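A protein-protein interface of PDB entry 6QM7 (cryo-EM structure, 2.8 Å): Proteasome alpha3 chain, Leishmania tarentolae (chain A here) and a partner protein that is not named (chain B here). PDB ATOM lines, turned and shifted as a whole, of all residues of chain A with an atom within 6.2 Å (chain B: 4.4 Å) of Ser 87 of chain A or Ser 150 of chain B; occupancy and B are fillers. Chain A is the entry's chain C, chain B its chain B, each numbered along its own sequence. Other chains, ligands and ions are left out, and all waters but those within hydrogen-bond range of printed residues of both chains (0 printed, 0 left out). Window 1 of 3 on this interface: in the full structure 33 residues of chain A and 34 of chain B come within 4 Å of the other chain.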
ATOM      1  N   GLY A  84      29.624 -25.888 -18.287  1.00  0.00           N
ATOM      2  CA  GLY A  84      28.265 -25.459 -18.647  1.00  0.00           C
ATOM      3  C   GLY A  84      27.876 -26.016 -19.998  1.00  0.00           C
ATOM      4  O   GLY A  84      28.321 -27.126 -20.337  1.00  0.00           O
ATOM      5  N   VAL A  85      27.083 -25.256 -20.744  1.00  0.00           N
ATOM      6  CA  VAL A  85      26.537 -25.643 -22.073  1.00  0.00           C
ATOM      7  C   VAL A  85      27.725 -25.824 -23.029  1.00  0.00           C
ATOM      8  O   VAL A  85      28.268 -24.805 -23.488  1.00  0.00           O
ATOM      9  CB  VAL A  85      25.535 -24.571 -22.556  1.00  0.00           C
ATOM     10  CG1 VAL A  85      24.889 -24.918 -23.896  1.00  0.00           C
ATOM     11  CG2 VAL A  85      24.476 -24.277 -21.499  1.00  0.00           C
ATOM     12  N   THR A  86      28.131 -27.068 -23.304  1.00  0.00           N
ATOM     13  CA  THR A  86      29.327 -27.386 -24.133  1.00  0.00           C
ATOM     14  C   THR A  86      29.222 -26.692 -25.493  1.00  0.00           C
ATOM     15  O   THR A  86      30.243 -26.209 -25.975  1.00  0.00           O
ATOM     16  CB  THR A  86      29.536 -28.893 -24.318  1.00  0.00           C
ATOM     17  OG1 THR A  86      28.316 -29.464 -24.796  1.00  0.00           O
ATOM     18  CG2 THR A  86      29.974 -29.585 -23.044  1.00  0.00           C
ATOM     19  N   SER A  87      28.030 -26.631 -26.078  1.00  0.00           N
ATOM     20  CA  SER A  87      27.789 -26.040 -27.417  1.00  0.00           C
ATOM     21  C   SER A  87      28.052 -24.526 -27.379  1.00  0.00           C
ATOM     22  O   SER A  87      28.596 -23.997 -28.368  1.00  0.00           O
ATOM     23  CB  SER A  87      26.397 -26.363 -27.906  1.00  0.00           C
ATOM     24  OG  SER A  87      26.062 -27.716 -27.615  1.00  0.00           O
ATOM     25  N   ASP A  88      27.684 -23.852 -26.285  1.00  0.00           N
ATOM     26  CA  ASP A  88      27.987 -22.413 -26.067  1.00  0.00           C
ATOM     27  C   ASP A  88      29.500 -22.254 -25.962  1.00  0.00           C
ATOM     28  O   ASP A  88      30.051 -21.381 -26.637  1.00  0.00           O
ATOM     29  CB  ASP A  88      27.333 -21.864 -24.795  1.00  0.00           C
ATOM     30  CG  ASP A  88      25.840 -21.572 -24.879  1.00  0.00           C
ATOM     31  OD1 ASP A  88      25.245 -21.730 -25.972  1.00  0.00           O
ATOM     32  OD2 ASP A  88      25.275 -21.189 -23.836  1.00  0.00           O
ATOM     33  N   ALA A  89      30.124 -23.081 -25.121  1.00  0.00           N
ATOM     34  CA  ALA A  89      31.589 -23.149 -24.929  1.00  0.00           C
ATOM     35  C   ALA A  89      32.292 -23.158 -26.284  1.00  0.00           C
ATOM     36  O   ALA A  89      33.184 -22.335 -26.465  1.00  0.00           O
ATOM     37  CB  ALA A  89      31.966 -24.357 -24.114  1.00  0.00           C
ATOM     38  N   TYR A  90      31.890 -24.048 -27.189  1.00  0.00           N
ATOM     39  CA  TYR A  90      32.511 -24.224 -28.530  1.00  0.00           C
ATOM     40  C   TYR A  90      32.386 -22.925 -29.328  1.00  0.00           C
ATOM     41  O   TYR A  90      33.365 -22.566 -30.011  1.00  0.00           O
ATOM     42  CB  TYR A  90      31.915 -25.410 -29.295  1.00  0.00           C
ATOM     43  CG  TYR A  90      32.593 -26.722 -28.996  1.00  0.00           C
ATOM     44  CD1 TYR A  90      33.828 -27.026 -29.555  1.00  0.00           C
ATOM     45  CD2 TYR A  90      32.016 -27.653 -28.145  1.00  0.00           C
ATOM     46  CE1 TYR A  90      34.471 -28.224 -29.276  1.00  0.00           C
ATOM     47  CE2 TYR A  90      32.646 -28.851 -27.848  1.00  0.00           C
ATOM     48  CZ  TYR A  90      33.876 -29.140 -28.417  1.00  0.00           C
ATOM     49  OH  TYR A  90      34.490 -30.327 -28.128  1.00  0.00           O
ATOM     50  N   ALA A  91      31.223 -22.271 -29.260  1.00  0.00           N
ATOM     51  CA  ALA A  91      30.915 -21.000 -29.957  1.00  0.00           C
ATOM     52  C   ALA A  91      31.901 -19.928 -29.504  1.00  0.00           C
ATOM     53  O   ALA A  91      32.456 -19.221 -30.369  1.00  0.00           O
ATOM     54  CB  ALA A  91      29.497 -20.558 -29.676  1.00  0.00           C
ATOM     55  N   LEU A  92      32.079 -19.820 -28.189  1.00  0.00           N
ATOM     56  CA  LEU A  92      32.942 -18.814 -27.527  1.00  0.00           C
ATOM     57  C   LEU A  92      34.404 -19.190 -27.689  1.00  0.00           C
ATOM     58  O   LEU A  92      35.223 -18.266 -27.830  1.00  0.00           O
ATOM     59  CB  LEU A  92      32.606 -18.752 -26.042  1.00  0.00           C
ATOM     60  CG  LEU A  92      31.397 -17.902 -25.691  1.00  0.00           C
ATOM     61  CD1 LEU A  92      31.184 -17.942 -24.201  1.00  0.00           C
ATOM     62  CD2 LEU A  92      31.560 -16.464 -26.179  1.00  0.00           C
ATOM     63  N   ILE B  20      15.577 -27.001 -25.338  1.00  0.00           N
ATOM     64  CA  ILE B  20      16.577 -27.980 -25.868  1.00  0.00           C
ATOM     65  C   ILE B  20      16.285 -29.367 -25.289  1.00  0.00           C
ATOM     66  O   ILE B  20      16.563 -30.349 -25.988  1.00  0.00           O
ATOM     67  CB  ILE B  20      18.019 -27.531 -25.560  1.00  0.00           C
ATOM     68  CG1 ILE B  20      18.334 -26.175 -26.190  1.00  0.00           C
ATOM     69  CG2 ILE B  20      19.034 -28.573 -25.999  1.00  0.00           C
ATOM     70  CD1 ILE B  20      19.609 -25.552 -25.673  1.00  0.00           C
ATOM     71  N   GLN B 117      23.529 -25.036 -32.374  1.00  0.00           N
ATOM     72  CA  GLN B 117      23.699 -24.101 -31.229  1.00  0.00           C
ATOM     73  C   GLN B 117      23.077 -22.762 -31.612  1.00  0.00           C
ATOM     74  O   GLN B 117      22.324 -22.246 -30.787  1.00  0.00           O
ATOM     75  CB  GLN B 117      25.162 -24.025 -30.756  1.00  0.00           C
ATOM     76  CG  GLN B 117      25.787 -22.621 -30.696  1.00  0.00           C
ATOM     77  CD  GLN B 117      25.415 -21.778 -29.497  1.00  0.00           C
ATOM     78  OE1 GLN B 117      25.515 -20.553 -29.536  1.00  0.00           O
ATOM     79  NE2 GLN B 117      25.005 -22.428 -28.418  1.00  0.00           N
ATOM     80  N   THR B 120      19.634 -22.744 -30.718  1.00  0.00           N
ATOM     81  CA  THR B 120      19.413 -22.782 -29.244  1.00  0.00           C
ATOM     82  C   THR B 120      19.601 -21.399 -28.609  1.00  0.00           C
ATOM     83  O   THR B 120      19.369 -21.306 -27.394  1.00  0.00           O
ATOM     84  CB  THR B 120      20.369 -23.755 -28.546  1.00  0.00           C
ATOM     85  OG1 THR B 120      21.697 -23.237 -28.606  1.00  0.00           O
ATOM     86  CG2 THR B 120      20.329 -25.146 -29.139  1.00  0.00           C
ATOM     87  N   ASP B 148      23.371 -33.722 -31.515  1.00  0.00           N
ATOM     88  CA  ASP B 148      22.059 -33.605 -30.816  1.00  0.00           C
ATOM     89  C   ASP B 148      21.518 -32.188 -30.934  1.00  0.00           C
ATOM     90  O   ASP B 148      22.251 -31.270 -31.285  1.00  0.00           O
ATOM     91  CB  ASP B 148      22.160 -34.035 -29.355  1.00  0.00           C
ATOM     92  CG  ASP B 148      22.045 -35.541 -29.190  1.00  0.00           C
ATOM     93  OD1 ASP B 148      20.953 -36.092 -29.489  1.00  0.00           O
ATOM     94  OD2 ASP B 148      23.061 -36.154 -28.791  1.00  0.00           O
ATOM     95  N   PRO B 149      20.206 -31.984 -30.688  1.00  0.00           N
ATOM     96  CA  PRO B 149      19.598 -30.650 -30.678  1.00  0.00           C
ATOM     97  C   PRO B 149      20.370 -29.558 -29.923  1.00  0.00           C
ATOM     98  O   PRO B 149      20.320 -28.412 -30.351  1.00  0.00           O
ATOM     99  CB  PRO B 149      18.281 -30.942 -29.962  1.00  0.00           C
ATOM    100  CG  PRO B 149      17.908 -32.277 -30.533  1.00  0.00           C
ATOM    101  CD  PRO B 149      19.211 -33.042 -30.455  1.00  0.00           C
ATOM    102  N   SER B 150      21.043 -29.947 -28.834  1.00  0.00           N
ATOM    103  CA  SER B 150      21.905 -29.092 -27.977  1.00  0.00           C
ATOM    104  C   SER B 150      23.043 -28.465 -28.786  1.00  0.00           C
ATOM    105  O   SER B 150      23.436 -27.329 -28.456  1.00  0.00           O
ATOM    106  CB  SER B 150      22.456 -29.889 -26.833  1.00  0.00           C
ATOM    107  OG  SER B 150      23.140 -31.033 -27.312  1.00  0.00           O
ATOM    108  N   GLY B 151      23.530 -29.173 -29.809  1.00  0.00           N
ATOM    109  CA  GLY B 151      24.775 -28.882 -30.540  1.00  0.00           C
ATOM    110  C   GLY B 151      25.856 -29.852 -30.113  1.00  0.00           C
ATOM    111  O   GLY B 151      26.913 -29.910 -30.775  1.00  0.00           O
ATOM    112  N   THR B 152      25.610 -30.594 -29.035  1.00  0.00           N
ATOM    113  CA  THR B 152      26.590 -31.532 -28.445  1.00  0.00           C
ATOM    114  C   THR B 152      26.805 -32.647 -29.457  1.00  0.00           C
ATOM    115  O   THR B 152      25.826 -33.071 -30.068  1.00  0.00           O
ATOM    116  CB  THR B 152      26.120 -32.052 -27.083  1.00  0.00           C
ATOM    117  OG1 THR B 152      25.966 -30.915 -26.235  1.00  0.00           O
ATOM    118  CG2 THR B 152      27.095 -33.033 -26.468  1.00  0.00           C
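The side-chain hydroxyl (OG1) of Thr 152 of chain B is in hydrogen-bond range of the side-chain hydroxyl (OG1) of Thr 86 of chain A (3.1 Å).
NE2 of Gln 117 of chain B is in hydrogen-bond range of OD1 of Asp 88 of chain A, 2.6 Å away.
O of Ser 150 of chain B is in hydrogen-bond range of OG of Ser 87 of chain A (2.8 Å).
The backbone NH of Thr 152 of chain B is in hydrogen-bond range of the side-chain hydroxyl of Ser 87 of chain A, 3.2 Å away.
The side-chain hydroxyl of Ser 150 of chain B is in hydrogen-bond range of the side-chain hydroxyl of Thr 152 of chain B (3.0 Å).
The backbone carbonyl oxygen of Gln 117 of chain B lies within hydrogen-bond range of the side-chain hydroxyl of Thr 120 of chain B, at 2.5 Å.
C of Ser 87 of chain A touches NE2 of Gln 117 of chain B (3.8 Å).
C of Gly 151 of chain B touches OG of Ser 87 of chain A, 3.3 Å away.
Gln 117 of chain B touches Ala 91 of chain A (OE1 to CB, 3.98 Å).
Ser 87 of chain A touches just these residues of chain B: Gln 117 (3.8 Å), Ser 150 (2.8 Å), Gly 151 (3.3 Å) and Thr 152 (3.2 Å).
Of the printed residues of chain B, Asp 88 of chain A touches Gln 117.
Printed residues of chain B within 4 Å of Ala 91 of chain A: Gln 117 (3.98 Å).
Of the printed residues of chain A, Gln 117 of chain B touches Ser 87 (3.8 Å), Asp 88 (2.6 Å) and Ala 91 (3.98 Å).
Ser 150 of chain B touches just one residue of chain A: Ser 87.
Of the printed residues of chain A, Gly 151 of chain B touches Ser 87.
The nearest printed residue of chain B that does not touch Ser 87 of chain A is Thr 120 of chain B (5.7 Å).
The nearest residue of chain A that does not touch Ser 150 of chain B is Val 85 of chain A (5.4 Å).
The nearest printed residue of chain A that does not touch Gly 151 of chain B is Thr 86 of chain A (5.9 Å).
Hydrophobic or aromatic side chains of chain A that line the printed part of chain B: Ala 91.
Printed residues of chain B that touch a printed residue of chain A: Gln 117, Ser 150, Gly 151 and Thr 152.
Along chain B the printed residues that touch a printed residue of chain A span positions 117 to 152.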
